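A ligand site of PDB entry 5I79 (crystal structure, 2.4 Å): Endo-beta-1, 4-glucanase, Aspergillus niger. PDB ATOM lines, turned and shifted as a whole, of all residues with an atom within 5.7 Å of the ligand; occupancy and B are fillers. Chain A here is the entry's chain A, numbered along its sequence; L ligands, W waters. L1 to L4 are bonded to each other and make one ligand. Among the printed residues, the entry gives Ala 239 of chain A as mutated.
O5 of LG4 L4 is in hydrogen-bond range of O of Asp 27.
OE2 of Glu 132 lies within hydrogen-bond range of O1 of LIG L1.
An oxygen (O5) of LG2 L2 is in hydrogen-bond range of the side-chain carboxylate (OE2) of Glu 15, 2.8 Å away.
OH of Tyr 199 sits at hydrogen-bond distance from O1 of LIG L1 (2.9 Å).
NE2 of His 92 lies close to O2 of LIG L1, at 3.2 Å.
O3 of LIG L1 lies within hydrogen-bond range of OH of Tyr 94, 3.0 Å away.
An oxygen (O6) of LIG L1 is in hydrogen-bond range of the backbone carbonyl oxygen (O) of Ser 205 (3.0 Å).
N of Gly 17 sits at hydrogen-bond distance from O1 of LG3 L3, 3.1 Å away.
ND2 of Asn 131 is in hydrogen-bond range of O2 of LIG L1 (3.1 Å).
The indole nitrogen of Trp 272 lies within hydrogen-bond range of an oxygen (O4) of LIG L1 (3.3 Å).
O of Gly 206 sits at hydrogen-bond distance from O6 of LIG L1 (3.4 Å).
ND2 of Asn 131 is in hydrogen-bond range of OE1 of Glu 132, 3.1 Å away.
The side-chain carboxylate of Glu 132 lies within hydrogen-bond range of a ring nitrogen (ND1) of His 197, at 2.5 Å.
NE2 of His 92 sits at hydrogen-bond distance from OD1 of Asn 131, 3.1 Å away.
The backbone NH (N) of Tyr 94 is in hydrogen-bond range of the backbone carbonyl oxygen (O) of Asn 131 (2.9 Å).
The side-chain hydroxyl (OG1) of Thr 207 lies within hydrogen-bond range of the side-chain hydroxyl (OG) of Ser 205 (2.7 Å).
The indole nitrogen (NE1) of Trp 272 is in hydrogen-bond range of the side-chain hydroxyl (OH) of Tyr 281 (3.1 Å).
Merely in contact with the ligand: Phe 16, Thr 26, His 197, Thr 207, Trp 277, Trp 278 and Tyr 281.
Hydrophobic or aromatic side chains that line the ligand: Phe 16, His 92, Tyr 94, Tyr 199, Trp 272, Trp 277 and Trp 278.
Of the 24 residues printed, 18 come within 4 Å of the ligand.
Along chain A the residues within 4 Å of the ligand span positions 15 to 281.
Water W1 lies within hydrogen-bond range of an oxygen (O5) of LG2 L2 (2.5 Å) and the side-chain hydroxyl of Tyr 94 (3.1 Å).
Water W2 lies within hydrogen-bond range of OD1 of Asn 131 (2.6 Å), O1 of LIG L1 (2.9 Å) and NE2 of His 92 (3.2 Å).
Water W3 lies within hydrogen-bond range of an oxygen (O5) of LG3 L3 and the backbone NH of Tyr 281.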
ATOM      1  N   SER A  12     -21.926  -9.571  16.146  1.00  0.00           N
ATOM      2  CA  SER A  12     -21.391  -9.020  14.938  1.00  0.00           C
ATOM      3  C   SER A  12     -21.625  -9.928  13.744  1.00  0.00           C
ATOM      4  O   SER A  12     -21.874 -11.140  13.876  1.00  0.00           O
ATOM      5  CB  SER A  12     -19.898  -8.839  15.154  1.00  0.00           C
ATOM      6  OG  SER A  12     -19.680  -8.518  16.539  1.00  0.00           O
ATOM      7  N   GLU A  15     -22.096  -6.195   9.738  1.00  0.00           N
ATOM      8  CA  GLU A  15     -21.151  -5.189   9.240  1.00  0.00           C
ATOM      9  C   GLU A  15     -19.927  -5.805   8.574  1.00  0.00           C
ATOM     10  O   GLU A  15     -18.960  -5.135   8.248  1.00  0.00           O
ATOM     11  CB  GLU A  15     -20.745  -4.232  10.374  1.00  0.00           C
ATOM     12  CG  GLU A  15     -19.624  -4.657  11.335  1.00  0.00           C
ATOM     13  CD  GLU A  15     -19.874  -5.904  12.160  1.00  0.00           C
ATOM     14  OE1 GLU A  15     -20.958  -6.551  12.030  1.00  0.00           O
ATOM     15  OE2 GLU A  15     -18.956  -6.244  12.943  1.00  0.00           O
ATOM     16  N   PHE A  16     -19.957  -7.115   8.380  1.00  0.00           N
ATOM     17  CA  PHE A  16     -18.748  -7.822   7.903  1.00  0.00           C
ATOM     18  C   PHE A  16     -18.448  -7.442   6.450  1.00  0.00           C
ATOM     19  O   PHE A  16     -19.328  -6.944   5.743  1.00  0.00           O
ATOM     20  CB  PHE A  16     -18.884  -9.367   8.074  1.00  0.00           C
ATOM     21  CG  PHE A  16     -18.440  -9.888   9.424  1.00  0.00           C
ATOM     22  CD1 PHE A  16     -18.436  -9.090  10.555  1.00  0.00           C
ATOM     23  CD2 PHE A  16     -18.061 -11.211   9.574  1.00  0.00           C
ATOM     24  CE1 PHE A  16     -18.051  -9.597  11.797  1.00  0.00           C
ATOM     25  CE2 PHE A  16     -17.652 -11.719  10.813  1.00  0.00           C
ATOM     26  CZ  PHE A  16     -17.661 -10.910  11.915  1.00  0.00           C
ATOM     27  N   GLY A  17     -17.200  -7.672   6.047  1.00  0.00           N
ATOM     28  CA  GLY A  17     -16.845  -7.758   4.638  1.00  0.00           C
ATOM     29  C   GLY A  17     -16.405  -6.426   4.062  1.00  0.00           C
ATOM     30  O   GLY A  17     -16.671  -5.367   4.628  1.00  0.00           O
ATOM     31  N   THR A  18     -15.721  -6.492   2.915  1.00  0.00           N
ATOM     32  CA  THR A  18     -15.202  -5.309   2.244  1.00  0.00           C
ATOM     33  C   THR A  18     -16.156  -4.783   1.161  1.00  0.00           C
ATOM     34  O   THR A  18     -16.081  -3.590   0.832  1.00  0.00           O
ATOM     35  CB  THR A  18     -13.811  -5.581   1.654  1.00  0.00           C
ATOM     36  OG1 THR A  18     -13.844  -6.789   0.882  1.00  0.00           O
ATOM     37  CG2 THR A  18     -12.735  -5.712   2.789  1.00  0.00           C
ATOM     38  N   THR A  26     -22.576 -14.168   1.676  1.00  0.00           N
ATOM     39  CA  THR A  26     -21.270 -14.118   1.042  1.00  0.00           C
ATOM     40  C   THR A  26     -20.371 -13.118   1.771  1.00  0.00           C
ATOM     41  O   THR A  26     -19.282 -13.463   2.211  1.00  0.00           O
ATOM     42  CB  THR A  26     -21.412 -13.617  -0.409  1.00  0.00           C
ATOM     43  OG1 THR A  26     -22.433 -14.370  -1.087  1.00  0.00           O
ATOM     44  CG2 THR A  26     -20.071 -13.717  -1.181  1.00  0.00           C
ATOM     45  N   ASP A  27     -20.838 -11.872   1.869  1.00  0.00           N
ATOM     46  CA  ASP A  27     -20.057 -10.767   2.385  1.00  0.00           C
ATOM     47  C   ASP A  27     -20.293 -10.542   3.855  1.00  0.00           C
ATOM     48  O   ASP A  27     -19.357 -10.173   4.576  1.00  0.00           O
ATOM     49  CB  ASP A  27     -20.427  -9.527   1.611  1.00  0.00           C
ATOM     50  CG  ASP A  27     -19.939  -9.572   0.157  1.00  0.00           C
ATOM     51  OD1 ASP A  27     -18.704  -9.589  -0.034  1.00  0.00           O
ATOM     52  OD2 ASP A  27     -20.788  -9.563  -0.776  1.00  0.00           O
ATOM     53  N   TYR A  28     -21.533 -10.775   4.297  1.00  0.00           N
ATOM     54  CA  TYR A  28     -21.976 -10.577   5.667  1.00  0.00           C
ATOM     55  C   TYR A  28     -23.156 -11.519   5.963  1.00  0.00           C
ATOM     56  O   TYR A  28     -23.638 -12.239   5.068  1.00  0.00           O
ATOM     57  CB  TYR A  28     -22.426  -9.123   5.885  1.00  0.00           C
ATOM     58  CG  TYR A  28     -23.662  -8.728   5.077  1.00  0.00           C
ATOM     59  CD1 TYR A  28     -24.942  -8.932   5.579  1.00  0.00           C
ATOM     60  CD2 TYR A  28     -23.532  -8.143   3.821  1.00  0.00           C
ATOM     61  CE1 TYR A  28     -26.076  -8.581   4.842  1.00  0.00           C
ATOM     62  CE2 TYR A  28     -24.652  -7.732   3.091  1.00  0.00           C
ATOM     63  CZ  TYR A  28     -25.916  -7.966   3.610  1.00  0.00           C
ATOM     64  OH  TYR A  28     -27.001  -7.554   2.893  1.00  0.00           O
ATOM     65  N   GLN A  50     -24.312  -5.076  15.832  1.00  0.00           N
ATOM     66  CA  GLN A  50     -23.637  -4.247  14.835  1.00  0.00           C
ATOM     67  C   GLN A  50     -24.452  -4.198  13.536  1.00  0.00           C
ATOM     68  O   GLN A  50     -25.030  -5.221  13.116  1.00  0.00           O
ATOM     69  CB  GLN A  50     -22.242  -4.823  14.508  1.00  0.00           C
ATOM     70  CG  GLN A  50     -21.105  -4.565  15.495  1.00  0.00           C
ATOM     71  CD  GLN A  50     -21.312  -5.276  16.794  1.00  0.00           C
ATOM     72  OE1 GLN A  50     -21.289  -6.504  16.844  1.00  0.00           O
ATOM     73  NE2 GLN A  50     -21.504  -4.519  17.867  1.00  0.00           N
ATOM     74  N   HIS A  92     -22.163   0.638  13.029  1.00  0.00           N
ATOM     75  CA  HIS A  92     -20.716   0.392  13.182  1.00  0.00           C
ATOM     76  C   HIS A  92     -19.879   1.103  12.116  1.00  0.00           C
ATOM     77  O   HIS A  92     -19.291   0.487  11.209  1.00  0.00           O
ATOM     78  CB  HIS A  92     -20.461  -1.132  13.163  1.00  0.00           C
ATOM     79  CG  HIS A  92     -19.379  -1.579  14.091  1.00  0.00           C
ATOM     80  ND1 HIS A  92     -18.177  -2.041  13.638  1.00  0.00           N
ATOM     81  CD2 HIS A  92     -19.334  -1.633  15.444  1.00  0.00           C
ATOM     82  CE1 HIS A  92     -17.411  -2.354  14.676  1.00  0.00           C
ATOM     83  NE2 HIS A  92     -18.093  -2.127  15.778  1.00  0.00           N
ATOM     84  N   TYR A  94     -17.875   4.433  12.659  1.00  0.00           N
ATOM     85  CA  TYR A  94     -16.680   5.216  12.987  1.00  0.00           C
ATOM     86  C   TYR A  94     -16.805   6.678  12.639  1.00  0.00           C
ATOM     87  O   TYR A  94     -15.896   7.304  12.163  1.00  0.00           O
ATOM     88  CB  TYR A  94     -15.474   4.587  12.286  1.00  0.00           C
ATOM     89  CG  TYR A  94     -15.308   3.082  12.529  1.00  0.00           C
ATOM     90  CD1 TYR A  94     -14.615   2.602  13.659  1.00  0.00           C
ATOM     91  CD2 TYR A  94     -15.798   2.160  11.640  1.00  0.00           C
ATOM     92  CE1 TYR A  94     -14.448   1.244  13.883  1.00  0.00           C
ATOM     93  CE2 TYR A  94     -15.638   0.797  11.869  1.00  0.00           C
ATOM     94  CZ  TYR A  94     -14.966   0.353  12.997  1.00  0.00           C
ATOM     95  OH  TYR A  94     -14.805  -0.984  13.210  1.00  0.00           O
ATOM     96  N   ASN A 131     -20.317   3.859  16.381  1.00  0.00           N
ATOM     97  CA  ASN A 131     -19.165   3.136  16.886  1.00  0.00           C
ATOM     98  C   ASN A 131     -17.865   3.842  16.599  1.00  0.00           C
ATOM     99  O   ASN A 131     -17.457   3.989  15.453  1.00  0.00           O
ATOM    100  CB  ASN A 131     -19.075   1.803  16.192  1.00  0.00           C
ATOM    101  CG  ASN A 131     -17.936   0.939  16.723  1.00  0.00           C
ATOM    102  OD1 ASN A 131     -18.096   0.308  17.776  1.00  0.00           O
ATOM    103  ND2 ASN A 131     -16.813   0.862  15.985  1.00  0.00           N
ATOM    104  N   GLU A 132     -17.171   4.241  17.658  1.00  0.00           N
ATOM    105  CA  GLU A 132     -15.771   4.671  17.580  1.00  0.00           C
ATOM    106  C   GLU A 132     -15.466   5.763  16.567  1.00  0.00           C
ATOM    107  O   GLU A 132     -14.911   5.495  15.519  1.00  0.00           O
ATOM    108  CB  GLU A 132     -14.881   3.450  17.342  1.00  0.00           C
ATOM    109  CG  GLU A 132     -14.944   2.501  18.514  1.00  0.00           C
ATOM    110  CD  GLU A 132     -14.221   1.201  18.265  1.00  0.00           C
ATOM    111  OE1 GLU A 132     -13.913   0.927  17.079  1.00  0.00           O
ATOM    112  OE2 GLU A 132     -14.000   0.453  19.271  1.00  0.00           O
ATOM    113  N   HIS A 197     -14.669   1.976  25.083  1.00  0.00           N
ATOM    114  CA  HIS A 197     -14.129   0.670  24.727  1.00  0.00           C
ATOM    115  C   HIS A 197     -12.752   0.488  25.330  1.00  0.00           C
ATOM    116  O   HIS A 197     -12.065   1.423  25.556  1.00  0.00           O
ATOM    117  CB  HIS A 197     -14.073   0.551  23.219  1.00  0.00           C
ATOM    118  CG  HIS A 197     -15.413   0.625  22.568  1.00  0.00           C
ATOM    119  ND1 HIS A 197     -15.568   0.689  21.202  1.00  0.00           N
ATOM    120  CD2 HIS A 197     -16.670   0.637  23.076  1.00  0.00           C
ATOM    121  CE1 HIS A 197     -16.854   0.763  20.902  1.00  0.00           C
ATOM    122  NE2 HIS A 197     -17.551   0.718  22.023  1.00  0.00           N
ATOM    123  N   TYR A 199      -9.351  -2.277  25.131  1.00  0.00           N
ATOM    124  CA  TYR A 199      -8.578  -3.462  24.907  1.00  0.00           C
ATOM    125  C   TYR A 199      -7.276  -3.399  25.699  1.00  0.00           C
ATOM    126  O   TYR A 199      -6.923  -2.358  26.231  1.00  0.00           O
ATOM    127  CB  TYR A 199      -8.343  -3.675  23.425  1.00  0.00           C
ATOM    128  CG  TYR A 199      -9.655  -3.859  22.678  1.00  0.00           C
ATOM    129  CD1 TYR A 199     -10.317  -5.044  22.708  1.00  0.00           C
ATOM    130  CD2 TYR A 199     -10.242  -2.806  21.950  1.00  0.00           C
ATOM    131  CE1 TYR A 199     -11.526  -5.218  22.036  1.00  0.00           C
ATOM    132  CE2 TYR A 199     -11.443  -2.976  21.273  1.00  0.00           C
ATOM    133  CZ  TYR A 199     -12.090  -4.190  21.320  1.00  0.00           C
ATOM    134  OH  TYR A 199     -13.296  -4.406  20.639  1.00  0.00           O
ATOM    135  N   SER A 205      -5.351  -1.783  20.395  1.00  0.00           N
ATOM    136  CA  SER A 205      -6.104  -2.024  19.151  1.00  0.00           C
ATOM    137  C   SER A 205      -6.994  -3.247  19.228  1.00  0.00           C
ATOM    138  O   SER A 205      -7.838  -3.465  18.356  1.00  0.00           O
ATOM    139  CB  SER A 205      -5.124  -2.270  17.998  1.00  0.00           C
ATOM    140  OG  SER A 205      -4.313  -3.427  18.252  1.00  0.00           O
ATOM    141  N   GLY A 206      -6.804  -4.072  20.229  1.00  0.00           N
ATOM    142  CA  GLY A 206      -7.603  -5.305  20.331  1.00  0.00           C
ATOM    143  C   GLY A 206      -7.332  -6.293  19.197  1.00  0.00           C
ATOM    144  O   GLY A 206      -8.223  -6.980  18.727  1.00  0.00           O
ATOM    145  N   THR A 207      -6.093  -6.364  18.732  1.00  0.00           N
ATOM    146  CA  THR A 207      -5.791  -7.268  17.627  1.00  0.00           C
ATOM    147  C   THR A 207      -4.795  -8.325  18.024  1.00  0.00           C
ATOM    148  O   THR A 207      -4.421  -9.079  17.203  1.00  0.00           O
ATOM    149  CB  THR A 207      -5.260  -6.520  16.410  1.00  0.00           C
ATOM    150  OG1 THR A 207      -4.130  -5.740  16.795  1.00  0.00           O
ATOM    151  CG2 THR A 207      -6.366  -5.589  15.825  1.00  0.00           C
ATOM    152  N   ALA A 239     -17.208  -2.530  24.437  1.00  0.00           N
ATOM    153  CA  ALA A 239     -16.375  -3.452  23.694  1.00  0.00           C
ATOM    154  C   ALA A 239     -15.067  -3.668  24.455  1.00  0.00           C
ATOM    155  O   ALA A 239     -14.397  -2.744  24.778  1.00  0.00           O
ATOM    156  CB  ALA A 239     -16.133  -2.972  22.291  1.00  0.00           C
ATOM    157  N   TRP A 272     -16.449  -8.077  23.245  1.00  0.00           N
ATOM    158  CA  TRP A 272     -16.234  -8.131  21.817  1.00  0.00           C
ATOM    159  C   TRP A 272     -15.599  -9.501  21.562  1.00  0.00           C
ATOM    160  O   TRP A 272     -14.432  -9.679  21.919  1.00  0.00           O
ATOM    161  CB  TRP A 272     -15.303  -6.995  21.361  1.00  0.00           C
ATOM    162  CG  TRP A 272     -15.164  -7.002  19.918  1.00  0.00           C
ATOM    163  CD1 TRP A 272     -14.194  -7.636  19.169  1.00  0.00           C
ATOM    164  CD2 TRP A 272     -16.072  -6.449  18.993  1.00  0.00           C
ATOM    165  NE1 TRP A 272     -14.460  -7.502  17.832  1.00  0.00           N
ATOM    166  CE2 TRP A 272     -15.612  -6.773  17.701  1.00  0.00           C
ATOM    167  CE3 TRP A 272     -17.233  -5.689  19.130  1.00  0.00           C
ATOM    168  CZ2 TRP A 272     -16.264  -6.364  16.575  1.00  0.00           C
ATOM    169  CZ3 TRP A 272     -17.881  -5.290  18.003  1.00  0.00           C
ATOM    170  CH2 TRP A 272     -17.397  -5.629  16.732  1.00  0.00           C
ATOM    171  N   TRP A 277     -20.083 -15.871  12.369  1.00  0.00           N
ATOM    172  CA  TRP A 277     -19.046 -15.999  11.382  1.00  0.00           C
ATOM    173  C   TRP A 277     -17.673 -15.614  11.918  1.00  0.00           C
ATOM    174  O   TRP A 277     -16.783 -15.281  11.165  1.00  0.00           O
ATOM    175  CB  TRP A 277     -19.376 -15.126  10.190  1.00  0.00           C
ATOM    176  CG  TRP A 277     -20.224 -15.781   9.156  1.00  0.00           C
ATOM    177  CD1 TRP A 277     -20.941 -16.916   9.277  1.00  0.00           C
ATOM    178  CD2 TRP A 277     -20.457 -15.295   7.828  1.00  0.00           C
ATOM    179  NE1 TRP A 277     -21.603 -17.197   8.110  1.00  0.00           N
ATOM    180  CE2 TRP A 277     -21.315 -16.215   7.195  1.00  0.00           C
ATOM    181  CE3 TRP A 277     -20.009 -14.177   7.104  1.00  0.00           C
ATOM    182  CZ2 TRP A 277     -21.767 -16.055   5.882  1.00  0.00           C
ATOM    183  CZ3 TRP A 277     -20.433 -14.019   5.809  1.00  0.00           C
ATOM    184  CH2 TRP A 277     -21.311 -14.963   5.204  1.00  0.00           C
ATOM    185  N   TRP A 278     -17.462 -15.711  13.226  1.00  0.00           N
ATOM    186  CA  TRP A 278     -16.136 -15.450  13.737  1.00  0.00           C
ATOM    187  C   TRP A 278     -15.174 -16.627  13.554  1.00  0.00           C
ATOM    188  O   TRP A 278     -13.989 -16.420  13.683  1.00  0.00           O
ATOM    189  CB  TRP A 278     -16.188 -15.082  15.212  1.00  0.00           C
ATOM    190  CG  TRP A 278     -16.676 -13.702  15.452  1.00  0.00           C
ATOM    191  CD1 TRP A 278     -17.820 -13.347  16.109  1.00  0.00           C
ATOM    192  CD2 TRP A 278     -16.040 -12.475  15.084  1.00  0.00           C
ATOM    193  NE1 TRP A 278     -17.948 -12.003  16.151  1.00  0.00           N
ATOM    194  CE2 TRP A 278     -16.861 -11.425  15.550  1.00  0.00           C
ATOM    195  CE3 TRP A 278     -14.851 -12.160  14.412  1.00  0.00           C
ATOM    196  CZ2 TRP A 278     -16.525 -10.069  15.367  1.00  0.00           C
ATOM    197  CZ3 TRP A 278     -14.511 -10.835  14.229  1.00  0.00           C
ATOM    198  CH2 TRP A 278     -15.348  -9.796  14.719  1.00  0.00           C
ATOM    199  N   TYR A 281     -11.680 -16.899  15.453  1.00  0.00           N
ATOM    200  CA  TYR A 281     -11.368 -15.627  16.080  1.00  0.00           C
ATOM    201  C   TYR A 281     -10.945 -15.787  17.520  1.00  0.00           C
ATOM    202  O   TYR A 281     -11.600 -16.494  18.283  1.00  0.00           O
ATOM    203  CB  TYR A 281     -12.591 -14.729  16.012  1.00  0.00           C
ATOM    204  CG  TYR A 281     -12.377 -13.276  16.343  1.00  0.00           C
ATOM    205  CD1 TYR A 281     -11.359 -12.556  15.772  1.00  0.00           C
ATOM    206  CD2 TYR A 281     -13.268 -12.618  17.218  1.00  0.00           C
ATOM    207  CE1 TYR A 281     -11.182 -11.213  16.081  1.00  0.00           C
ATOM    208  CE2 TYR A 281     -13.113 -11.295  17.520  1.00  0.00           C
ATOM    209  CZ  TYR A 281     -12.064 -10.586  16.965  1.00  0.00           C
ATOM    210  OH  TYR A 281     -11.931  -9.252  17.282  1.00  0.00           O
ATOM    211  N   PHE A 283     -11.241 -13.902  19.986  1.00  0.00           N
ATOM    212  CA  PHE A 283     -12.169 -13.332  20.968  1.00  0.00           C
ATOM    213  C   PHE A 283     -13.600 -13.833  20.858  1.00  0.00           C
ATOM    214  O   PHE A 283     -14.520 -13.227  21.433  1.00  0.00           O
ATOM    215  CB  PHE A 283     -12.135 -11.796  20.854  1.00  0.00           C
ATOM    216  CG  PHE A 283     -10.805 -11.188  21.127  1.00  0.00           C
ATOM    217  CD1 PHE A 283      -9.992 -11.656  22.152  1.00  0.00           C
ATOM    218  CD2 PHE A 283     -10.367 -10.088  20.412  1.00  0.00           C
ATOM    219  CE1 PHE A 283      -8.745 -11.072  22.422  1.00  0.00           C
ATOM    220  CE2 PHE A 283      -9.117  -9.491  20.678  1.00  0.00           C
ATOM    221  CZ  PHE A 283      -8.311  -9.992  21.688  1.00  0.00           C
HETATM  222  C1  LIG L   1     -13.842  -2.388  16.447  1.00  0.00           C
HETATM  223  C2  LIG L   1     -13.992  -3.785  15.727  1.00  0.00           C
HETATM  224  C3  LIG L   1     -12.620  -4.536  15.885  1.00  0.00           C
HETATM  225  C4  LIG L   1     -12.308  -4.521  17.377  1.00  0.00           C
HETATM  226  C5  LIG L   1     -11.066  -5.171  17.801  1.00  0.00           C
HETATM  227  C6  LIG L   1     -13.620  -2.885  17.881  1.00  0.00           C
HETATM  228  O1  LIG L   1     -14.097  -2.157  18.930  1.00  0.00           O
HETATM  229  O2  LIG L   1     -14.986  -1.607  16.291  1.00  0.00           O
HETATM  230  O3  LIG L   1     -14.483  -3.732  14.430  1.00  0.00           O
HETATM  231  O4  LIG L   1     -12.744  -5.939  15.474  1.00  0.00           O
HETATM  232  O5  LIG L   1     -12.266  -3.148  17.894  1.00  0.00           O
HETATM  233  O6  LIG L   1     -10.111  -4.807  16.880  1.00  0.00           O
HETATM  234  C1  LG2 L   2     -11.953  -7.402  13.811  1.00  0.00           C
HETATM  235  C2  LG2 L   2     -12.118  -7.777  12.349  1.00  0.00           C
HETATM  236  C3  LG2 L   2     -13.610  -7.797  11.956  1.00  0.00           C
HETATM  237  C4  LG2 L   2     -14.302  -6.539  12.419  1.00  0.00           C
HETATM  238  C5  LG2 L   2     -15.818  -6.649  12.390  1.00  0.00           C
HETATM  239  C6  LG2 L   2     -12.652  -6.117  14.083  1.00  0.00           C
HETATM  240  O1  LG2 L   2     -10.604  -7.212  14.134  1.00  0.00           O
HETATM  241  O2  LG2 L   2     -11.572  -9.043  12.104  1.00  0.00           O
HETATM  242  O3  LG2 L   2     -13.667  -7.836  10.537  1.00  0.00           O
HETATM  243  O4  LG2 L   2     -14.014  -6.298  13.804  1.00  0.00           O
HETATM  244  O5  LG2 L   2     -16.321  -5.317  12.538  1.00  0.00           O
HETATM  245  C1  LG3 L   3     -14.305  -8.933   8.633  1.00  0.00           C
HETATM  246  C2  LG3 L   3     -14.898 -10.183   8.081  1.00  0.00           C
HETATM  247  C3  LG3 L   3     -14.126 -11.401   8.477  1.00  0.00           C
HETATM  248  C4  LG3 L   3     -13.724 -11.390   9.959  1.00  0.00           C
HETATM  249  C5  LG3 L   3     -12.436 -12.256  10.065  1.00  0.00           C
HETATM  250  C6  LG3 L   3     -14.201  -9.056  10.088  1.00  0.00           C
HETATM  251  O1  LG3 L   3     -15.266  -7.890   8.420  1.00  0.00           O
HETATM  252  O2  LG3 L   3     -14.950 -10.103   6.682  1.00  0.00           O
HETATM  253  O3  LG3 L   3     -14.973 -12.564   8.290  1.00  0.00           O
HETATM  254  O4  LG3 L   3     -13.293 -10.060  10.403  1.00  0.00           O
HETATM  255  O5  LG3 L   3     -12.546 -13.065  11.203  1.00  0.00           O
HETATM  256  C1  LG4 L   4     -14.945 -14.651   7.138  1.00  0.00           C
HETATM  257  C2  LG4 L   4     -14.849 -15.246   5.758  1.00  0.00           C
HETATM  258  C3  LG4 L   4     -15.971 -14.627   4.883  1.00  0.00           C
HETATM  259  C4  LG4 L   4     -15.826 -13.092   4.865  1.00  0.00           C
HETATM  260  C5  LG4 L   4     -17.110 -12.484   4.317  1.00  0.00           C
HETATM  261  C6  LG4 L   4     -14.719 -13.179   7.037  1.00  0.00           C
HETATM  262  O1  LG4 L   4     -13.898 -15.205   7.885  1.00  0.00           O
HETATM  263  O2  LG4 L   4     -14.979 -16.646   5.931  1.00  0.00           O
HETATM  264  O3  LG4 L   4     -15.910 -15.089   3.535  1.00  0.00           O
HETATM  265  O4  LG4 L   4     -15.682 -12.575   6.203  1.00  0.00           O
HETATM  266  O5  LG4 L   4     -16.959 -11.061   4.465  1.00  0.00           O
HETATM  267  O   HOH W   1     -15.689  -3.200  11.268  1.00  0.00           O
HETATM  268  O   HOH W   2     -17.001  -1.905  18.730  1.00  0.00           O
HETATM  269  O   HOH W   3     -10.493 -15.185  12.668  1.00  0.00           O
HETATM  270  O   HOH W   4      -8.572  -8.433  12.666  1.00  0.00           O
